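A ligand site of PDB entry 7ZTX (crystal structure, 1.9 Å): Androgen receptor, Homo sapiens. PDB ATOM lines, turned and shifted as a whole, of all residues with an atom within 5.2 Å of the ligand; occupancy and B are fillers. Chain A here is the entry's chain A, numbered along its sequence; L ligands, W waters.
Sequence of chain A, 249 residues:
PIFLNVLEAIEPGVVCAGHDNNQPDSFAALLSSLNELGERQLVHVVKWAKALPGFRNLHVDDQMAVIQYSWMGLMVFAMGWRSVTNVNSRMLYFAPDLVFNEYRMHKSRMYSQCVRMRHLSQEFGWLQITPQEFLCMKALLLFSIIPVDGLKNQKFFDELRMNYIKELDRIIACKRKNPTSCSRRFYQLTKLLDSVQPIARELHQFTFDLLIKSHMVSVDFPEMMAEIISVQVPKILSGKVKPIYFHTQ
The side-chain amide oxygen of Asn 35 lies within hydrogen-bond range of an oxygen (O2) of the ligand (2.6 Å).
OG1 of Thr 207 is in hydrogen-bond range of O2 of the ligand.
The guanidinium group (NH2) of Arg 82 sits at hydrogen-bond distance from an oxygen (O1) of the ligand, at 3.0 Å.
The side-chain amide nitrogen of Gln 41 is in hydrogen-bond range of an oxygen (O1) of the ligand, at 3.5 Å.
The side-chain amide nitrogen (ND2) of Asn 35 sits close to the backbone carbonyl oxygen (O) of Leu 31 (3.4 Å).
NH2 of Arg 82 lies close to NE2 of Gln 41, 3.4 Å away.
The guanidinium group (NH2) of Arg 82 lies within hydrogen-bond range of the backbone carbonyl oxygen (O) of Phe 94, 2.8 Å away.
The side-chain amide oxygen of Gln 41 sits close to the side-chain sulfur of Met 75.
Residues that only touch the ligand: Leu 31 (3.95 Å), Leu 34 (3.4 Å), Leu 37 (3.9 Å), Met 72 (3.7 Å), Met 75 (3.6 Å), Val 76 (3.9 Å), Met 79 (3.7 Å), Phe 94 (3.7 Å), Phe 206 (3.8 Å) and Phe 221 (3.9 Å).
Hydrophobic or aromatic side chains that line the ligand: Leu 31, Leu 37, Met 72, Met 75, Val 76, Met 79, Phe 94, Phe 206 and Phe 221.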
ATOM      1  N   LEU A  31      -4.086 -12.326  29.618  1.00  0.00           N
ATOM      2  CA  LEU A  31      -4.291 -10.945  29.250  1.00  0.00           C
ATOM      3  C   LEU A  31      -3.126 -10.347  28.457  1.00  0.00           C
ATOM      4  O   LEU A  31      -3.384  -9.571  27.558  1.00  0.00           O
ATOM      5  CB  LEU A  31      -4.662 -10.112  30.488  1.00  0.00           C
ATOM      6  CG  LEU A  31      -6.158  -9.956  30.713  1.00  0.00           C
ATOM      7  CD1 LEU A  31      -6.816  -9.262  29.527  1.00  0.00           C
ATOM      8  CD2 LEU A  31      -6.794 -11.304  30.986  1.00  0.00           C
ATOM      9  N   LEU A  34      -3.818 -11.612  25.058  1.00  0.00           N
ATOM     10  CA  LEU A  34      -4.896 -10.925  24.369  1.00  0.00           C
ATOM     11  C   LEU A  34      -4.397  -9.575  23.860  1.00  0.00           C
ATOM     12  O   LEU A  34      -4.748  -9.156  22.768  1.00  0.00           O
ATOM     13  CB  LEU A  34      -6.076 -10.770  25.318  1.00  0.00           C
ATOM     14  CG  LEU A  34      -6.966 -12.001  25.484  1.00  0.00           C
ATOM     15  CD1 LEU A  34      -7.942 -11.813  26.650  1.00  0.00           C
ATOM     16  CD2 LEU A  34      -7.757 -12.263  24.216  1.00  0.00           C
ATOM     17  N   ASN A  35      -3.517  -8.935  24.644  1.00  0.00           N
ATOM     18  CA  ASN A  35      -2.977  -7.632  24.272  1.00  0.00           C
ATOM     19  C   ASN A  35      -2.104  -7.784  23.036  1.00  0.00           C
ATOM     20  O   ASN A  35      -2.144  -6.952  22.129  1.00  0.00           O
ATOM     21  CB  ASN A  35      -2.228  -6.935  25.426  1.00  0.00           C
ATOM     22  CG  ASN A  35      -3.144  -6.395  26.502  1.00  0.00           C
ATOM     23  OD1 ASN A  35      -4.281  -5.979  26.254  1.00  0.00           O
ATOM     24  ND2 ASN A  35      -2.612  -6.304  27.704  1.00  0.00           N
ATOM     25  N   LEU A  37      -2.288 -10.130  20.765  1.00  0.00           N
ATOM     26  CA  LEU A  37      -3.271 -10.359  19.711  1.00  0.00           C
ATOM     27  C   LEU A  37      -3.913  -9.046  19.246  1.00  0.00           C
ATOM     28  O   LEU A  37      -4.141  -8.864  18.051  1.00  0.00           O
ATOM     29  CB  LEU A  37      -4.371 -11.291  20.212  1.00  0.00           C
ATOM     30  CG  LEU A  37      -5.393 -11.633  19.130  1.00  0.00           C
ATOM     31  CD1 LEU A  37      -4.720 -12.299  17.892  1.00  0.00           C
ATOM     32  CD2 LEU A  37      -6.466 -12.544  19.685  1.00  0.00           C
ATOM     33  N   GLY A  38      -4.284  -8.182  20.194  1.00  0.00           N
ATOM     34  CA  GLY A  38      -4.882  -6.926  19.803  1.00  0.00           C
ATOM     35  C   GLY A  38      -3.941  -6.125  18.905  1.00  0.00           C
ATOM     36  O   GLY A  38      -4.377  -5.573  17.921  1.00  0.00           O
ATOM     37  N   GLN A  41      -3.727  -7.728  15.454  1.00  0.00           N
ATOM     38  CA  GLN A  41      -4.929  -7.533  14.651  1.00  0.00           C
ATOM     39  C   GLN A  41      -5.057  -6.059  14.240  1.00  0.00           C
ATOM     40  O   GLN A  41      -5.621  -5.776  13.195  1.00  0.00           O
ATOM     41  CB  GLN A  41      -6.180  -8.035  15.372  1.00  0.00           C
ATOM     42  CG  GLN A  41      -6.293  -9.556  15.425  1.00  0.00           C
ATOM     43  CD  GLN A  41      -7.622  -9.978  15.995  1.00  0.00           C
ATOM     44  OE1 GLN A  41      -8.563  -9.196  16.057  1.00  0.00           O
ATOM     45  NE2 GLN A  41      -7.723 -11.226  16.414  1.00  0.00           N
ATOM     46  N   TRP A  71     -11.705   0.153  16.666  1.00  0.00           N
ATOM     47  CA  TRP A  71     -11.067  -1.145  16.527  1.00  0.00           C
ATOM     48  C   TRP A  71     -11.670  -2.166  17.503  1.00  0.00           C
ATOM     49  O   TRP A  71     -11.717  -3.339  17.194  1.00  0.00           O
ATOM     50  CB  TRP A  71      -9.538  -1.058  16.712  1.00  0.00           C
ATOM     51  CG  TRP A  71      -9.158  -0.459  18.020  1.00  0.00           C
ATOM     52  CD1 TRP A  71      -8.988   0.866  18.294  1.00  0.00           C
ATOM     53  CD2 TRP A  71      -8.974  -1.150  19.280  1.00  0.00           C
ATOM     54  NE1 TRP A  71      -8.692   1.060  19.618  1.00  0.00           N
ATOM     55  CE2 TRP A  71      -8.678  -0.163  20.243  1.00  0.00           C
ATOM     56  CE3 TRP A  71      -9.004  -2.491  19.673  1.00  0.00           C
ATOM     57  CZ2 TRP A  71      -8.425  -0.493  21.584  1.00  0.00           C
ATOM     58  CZ3 TRP A  71      -8.739  -2.818  20.993  1.00  0.00           C
ATOM     59  CH2 TRP A  71      -8.443  -1.817  21.938  1.00  0.00           C
ATOM     60  N   MET A  72     -12.043  -1.741  18.703  1.00  0.00           N
ATOM     61  CA  MET A  72     -12.509  -2.727  19.680  1.00  0.00           C
ATOM     62  C   MET A  72     -13.789  -3.397  19.191  1.00  0.00           C
ATOM     63  O   MET A  72     -13.914  -4.625  19.239  1.00  0.00           O
ATOM     64  CB  MET A  72     -12.786  -2.103  21.055  1.00  0.00           C
ATOM     65  CG  MET A  72     -13.382  -3.118  22.042  1.00  0.00           C
ATOM     66  SD  MET A  72     -11.980  -4.059  22.638  1.00  0.00           S
ATOM     67  CE  MET A  72     -11.215  -2.910  23.801  1.00  0.00           C
ATOM     68  N   MET A  75     -12.983  -5.707  16.180  1.00  0.00           N
ATOM     69  CA  MET A  75     -12.301  -6.947  16.485  1.00  0.00           C
ATOM     70  C   MET A  75     -13.225  -7.908  17.223  1.00  0.00           C
ATOM     71  O   MET A  75     -13.086  -9.123  17.058  1.00  0.00           O
ATOM     72  CB  MET A  75     -11.045  -6.730  17.318  1.00  0.00           C
ATOM     73  CG  MET A  75     -10.020  -5.937  16.552  1.00  0.00           C
ATOM     74  SD  MET A  75      -8.614  -5.797  17.602  1.00  0.00           S
ATOM     75  CE  MET A  75      -7.620  -4.736  16.551  1.00  0.00           C
ATOM     76  N   VAL A  76     -14.176  -7.351  17.994  1.00  0.00           N
ATOM     77  CA  VAL A  76     -15.059  -8.185  18.788  1.00  0.00           C
ATOM     78  C   VAL A  76     -16.071  -8.830  17.863  1.00  0.00           C
ATOM     79  O   VAL A  76     -16.430  -9.987  18.060  1.00  0.00           O
ATOM     80  CB  VAL A  76     -15.733  -7.355  19.902  1.00  0.00           C
ATOM     81  CG1 VAL A  76     -17.009  -7.982  20.412  1.00  0.00           C
ATOM     82  CG2 VAL A  76     -14.752  -7.167  21.032  1.00  0.00           C
ATOM     83  N   MET A  79     -14.491 -11.541  16.015  1.00  0.00           N
ATOM     84  CA  MET A  79     -14.150 -12.628  16.902  1.00  0.00           C
ATOM     85  C   MET A  79     -15.404 -13.463  17.116  1.00  0.00           C
ATOM     86  O   MET A  79     -15.323 -14.703  17.140  1.00  0.00           O
ATOM     87  CB  MET A  79     -13.596 -12.108  18.241  1.00  0.00           C
ATOM     88  CG  MET A  79     -13.153 -13.219  19.181  1.00  0.00           C
ATOM     89  SD  MET A  79     -14.594 -13.895  20.112  1.00  0.00           S
ATOM     90  CE  MET A  79     -14.982 -12.483  21.175  1.00  0.00           C
ATOM     91  N   ARG A  82     -15.865 -15.639  13.951  1.00  0.00           N
ATOM     92  CA  ARG A  82     -14.945 -16.752  14.027  1.00  0.00           C
ATOM     93  C   ARG A  82     -15.484 -17.808  14.982  1.00  0.00           C
ATOM     94  O   ARG A  82     -15.308 -18.996  14.746  1.00  0.00           O
ATOM     95  CB  ARG A  82     -13.616 -16.308  14.637  1.00  0.00           C
ATOM     96  CG  ARG A  82     -12.788 -15.501  13.657  1.00  0.00           C
ATOM     97  CD  ARG A  82     -11.320 -15.528  14.060  1.00  0.00           C
ATOM     98  NE  ARG A  82     -11.043 -14.818  15.308  1.00  0.00           N
ATOM     99  CZ  ARG A  82     -10.983 -13.483  15.419  1.00  0.00           C
ATOM    100  NH1 ARG A  82     -11.219 -12.727  14.364  1.00  0.00           N
ATOM    101  NH2 ARG A  82     -10.682 -12.925  16.585  1.00  0.00           N
ATOM    102  N   PHE A  94     -10.638 -16.329  20.042  1.00  0.00           N
ATOM    103  CA  PHE A  94      -9.839 -15.132  19.842  1.00  0.00           C
ATOM    104  C   PHE A  94      -8.833 -15.372  18.698  1.00  0.00           C
ATOM    105  O   PHE A  94      -8.682 -14.550  17.796  1.00  0.00           O
ATOM    106  CB  PHE A  94      -9.188 -14.730  21.163  1.00  0.00           C
ATOM    107  CG  PHE A  94     -10.163 -14.233  22.218  1.00  0.00           C
ATOM    108  CD1 PHE A  94     -10.830 -13.028  22.060  1.00  0.00           C
ATOM    109  CD2 PHE A  94     -10.383 -14.958  23.375  1.00  0.00           C
ATOM    110  CE1 PHE A  94     -11.708 -12.568  23.036  1.00  0.00           C
ATOM    111  CE2 PHE A  94     -11.265 -14.484  24.355  1.00  0.00           C
ATOM    112  CZ  PHE A  94     -11.946 -13.292  24.175  1.00  0.00           C
ATOM    113  N   MET A 110     -12.733 -11.616  33.292  1.00  0.00           N
ATOM    114  CA  MET A 110     -13.479 -10.896  32.274  1.00  0.00           C
ATOM    115  C   MET A 110     -14.755 -11.671  32.041  1.00  0.00           C
ATOM    116  O   MET A 110     -15.271 -11.683  30.921  1.00  0.00           O
ATOM    117  CB  MET A 110     -12.752 -10.944  30.934  1.00  0.00           C
ATOM    118  CG  MET A 110     -11.536 -10.085  30.845  1.00  0.00           C
ATOM    119  SD  MET A 110     -11.416  -9.555  29.109  1.00  0.00           S
ATOM    120  CE  MET A 110     -10.734 -11.027  28.380  1.00  0.00           C
ATOM    121  N   MET A 117     -19.829 -11.140  24.893  1.00  0.00           N
ATOM    122  CA  MET A 117     -19.295 -11.470  23.582  1.00  0.00           C
ATOM    123  C   MET A 117     -19.883 -12.779  23.038  1.00  0.00           C
ATOM    124  O   MET A 117     -20.164 -12.916  21.840  1.00  0.00           O
ATOM    125  CB  MET A 117     -17.771 -11.563  23.643  1.00  0.00           C
ATOM    126  CG  MET A 117     -17.175 -10.218  23.967  1.00  0.00           C
ATOM    127  SD  MET A 117     -15.398 -10.193  23.843  1.00  0.00           S
ATOM    128  CE  MET A 117     -14.964 -10.710  25.508  1.00  0.00           C
ATOM    129  N   LEU A 203     -15.548  -3.374  27.297  1.00  0.00           N
ATOM    130  CA  LEU A 203     -14.176  -3.811  27.121  1.00  0.00           C
ATOM    131  C   LEU A 203     -13.222  -2.614  27.242  1.00  0.00           C
ATOM    132  O   LEU A 203     -12.079  -2.771  27.656  1.00  0.00           O
ATOM    133  CB  LEU A 203     -14.111  -4.500  25.736  1.00  0.00           C
ATOM    134  CG  LEU A 203     -14.726  -5.907  25.735  1.00  0.00           C
ATOM    135  CD1 LEU A 203     -14.856  -6.485  24.343  1.00  0.00           C
ATOM    136  CD2 LEU A 203     -13.939  -6.864  26.636  1.00  0.00           C
ATOM    137  N   PHE A 206     -12.628  -1.951  30.723  1.00  0.00           N
ATOM    138  CA  PHE A 206     -11.825  -3.006  31.321  1.00  0.00           C
ATOM    139  C   PHE A 206     -10.348  -2.833  30.947  1.00  0.00           C
ATOM    140  O   PHE A 206      -9.455  -2.909  31.774  1.00  0.00           O
ATOM    141  CB  PHE A 206     -12.375  -4.364  30.869  1.00  0.00           C
ATOM    142  CG  PHE A 206     -11.664  -5.507  31.527  1.00  0.00           C
ATOM    143  CD1 PHE A 206     -10.551  -6.079  30.937  1.00  0.00           C
ATOM    144  CD2 PHE A 206     -12.072  -5.969  32.767  1.00  0.00           C
ATOM    145  CE1 PHE A 206      -9.879  -7.127  31.549  1.00  0.00           C
ATOM    146  CE2 PHE A 206     -11.401  -7.021  33.393  1.00  0.00           C
ATOM    147  CZ  PHE A 206     -10.307  -7.585  32.781  1.00  0.00           C
ATOM    148  N   THR A 207     -10.096  -2.546  29.662  1.00  0.00           N
ATOM    149  CA  THR A 207      -8.708  -2.425  29.217  1.00  0.00           C
ATOM    150  C   THR A 207      -8.063  -1.156  29.796  1.00  0.00           C
ATOM    151  O   THR A 207      -6.850  -1.118  30.059  1.00  0.00           O
ATOM    152  CB  THR A 207      -8.592  -2.502  27.697  1.00  0.00           C
ATOM    153  OG1 THR A 207      -7.195  -2.707  27.454  1.00  0.00           O
ATOM    154  CG2 THR A 207      -9.000  -1.235  26.980  1.00  0.00           C
ATOM    155  N   LEU A 210      -7.093  -1.852  33.238  1.00  0.00           N
ATOM    156  CA  LEU A 210      -6.011  -2.813  33.291  1.00  0.00           C
ATOM    157  C   LEU A 210      -4.727  -2.079  32.939  1.00  0.00           C
ATOM    158  O   LEU A 210      -3.681  -2.444  33.445  1.00  0.00           O
ATOM    159  CB  LEU A 210      -6.291  -3.935  32.260  1.00  0.00           C
ATOM    160  CG  LEU A 210      -5.321  -5.107  32.252  1.00  0.00           C
ATOM    161  CD1 LEU A 210      -4.999  -5.584  33.659  1.00  0.00           C
ATOM    162  CD2 LEU A 210      -5.910  -6.250  31.459  1.00  0.00           C
ATOM    163  N   PHE A 221       1.494  -4.490  27.878  1.00  0.00           N
ATOM    164  CA  PHE A 221       0.776  -3.785  26.841  1.00  0.00           C
ATOM    165  C   PHE A 221       1.807  -3.412  25.771  1.00  0.00           C
ATOM    166  O   PHE A 221       2.705  -2.624  26.045  1.00  0.00           O
ATOM    167  CB  PHE A 221       0.086  -2.548  27.427  1.00  0.00           C
ATOM    168  CG  PHE A 221      -1.249  -2.805  28.078  1.00  0.00           C
ATOM    169  CD1 PHE A 221      -1.316  -3.223  29.399  1.00  0.00           C
ATOM    170  CD2 PHE A 221      -2.444  -2.666  27.383  1.00  0.00           C
ATOM    171  CE1 PHE A 221      -2.546  -3.494  30.007  1.00  0.00           C
ATOM    172  CE2 PHE A 221      -3.671  -2.904  27.988  1.00  0.00           C
ATOM    173  CZ  PHE A 221      -3.716  -3.298  29.327  1.00  0.00           C
ATOM    174  N   MET A 225      -0.766  -0.406  21.601  1.00  0.00           N
ATOM    175  CA  MET A 225      -1.939  -0.636  22.424  1.00  0.00           C
ATOM    176  C   MET A 225      -1.979   0.410  23.545  1.00  0.00           C
ATOM    177  O   MET A 225      -3.025   1.002  23.780  1.00  0.00           O
ATOM    178  CB  MET A 225      -1.901  -2.033  23.058  1.00  0.00           C
ATOM    179  CG  MET A 225      -2.204  -3.151  22.086  1.00  0.00           C
ATOM    180  SD  MET A 225      -3.877  -3.002  21.415  1.00  0.00           S
ATOM    181  CE  MET A 225      -4.810  -3.737  22.765  1.00  0.00           C
ATOM    182  N   ILE A 229      -4.937   3.187  24.117  1.00  0.00           N
ATOM    183  CA  ILE A 229      -5.774   3.047  25.285  1.00  0.00           C
ATOM    184  C   ILE A 229      -5.627   4.272  26.206  1.00  0.00           C
ATOM    185  O   ILE A 229      -6.532   4.587  26.956  1.00  0.00           O
ATOM    186  CB  ILE A 229      -5.520   1.698  25.983  1.00  0.00           C
ATOM    187  CG1 ILE A 229      -5.878   0.525  25.055  1.00  0.00           C
ATOM    188  CG2 ILE A 229      -6.236   1.611  27.344  1.00  0.00           C
ATOM    189  CD1 ILE A 229      -5.345  -0.816  25.524  1.00  0.00           C
HETATM  190  C1  LIG L   1      -8.175  -8.974  20.794  1.00  0.00           C
HETATM  191  C2  LIG L   1      -8.723  -9.360  19.405  1.00  0.00           C
HETATM  192  C3  LIG L   1      -9.979 -10.164  19.524  1.00  0.00           C
HETATM  193  O1  LIG L   1     -10.090 -11.230  18.940  1.00  0.00           O
HETATM  194  C4  LIG L   1     -11.058  -9.614  20.432  1.00  0.00           C
HETATM  195  C5  LIG L   1     -10.475  -9.161  21.766  1.00  0.00           C
HETATM  196  C6  LIG L   1     -11.523  -8.657  22.750  1.00  0.00           C
HETATM  197  C7  LIG L   1     -10.882  -8.455  24.128  1.00  0.00           C
HETATM  198  C8  LIG L   1      -9.699  -7.475  24.042  1.00  0.00           C
HETATM  199  C9  LIG L   1      -8.630  -7.927  23.039  1.00  0.00           C
HETATM  200  C10 LIG L   1      -9.229  -8.229  21.630  1.00  0.00           C
HETATM  201  C11 LIG L   1      -7.391  -7.005  23.019  1.00  0.00           C
HETATM  202  C12 LIG L   1      -6.780  -6.829  24.423  1.00  0.00           C
HETATM  203  C13 LIG L   1      -7.856  -6.315  25.372  1.00  0.00           C
HETATM  204  C14 LIG L   1      -9.014  -7.304  25.389  1.00  0.00           C
HETATM  205  C15 LIG L   1      -9.861  -6.827  26.584  1.00  0.00           C
HETATM  206  C16 LIG L   1      -8.796  -6.420  27.625  1.00  0.00           C
HETATM  207  C17 LIG L   1      -7.468  -6.376  26.855  1.00  0.00           C
HETATM  208  O2  LIG L   1      -6.609  -5.354  27.305  1.00  0.00           O
HETATM  209  C18 LIG L   1      -8.295  -4.893  24.962  1.00  0.00           C
HETATM  210  C19 LIG L   1      -9.600  -6.926  20.883  1.00  0.00           C
HETATM  211  O   HOH W   1     -10.872  -9.963  15.788  1.00  0.00           O
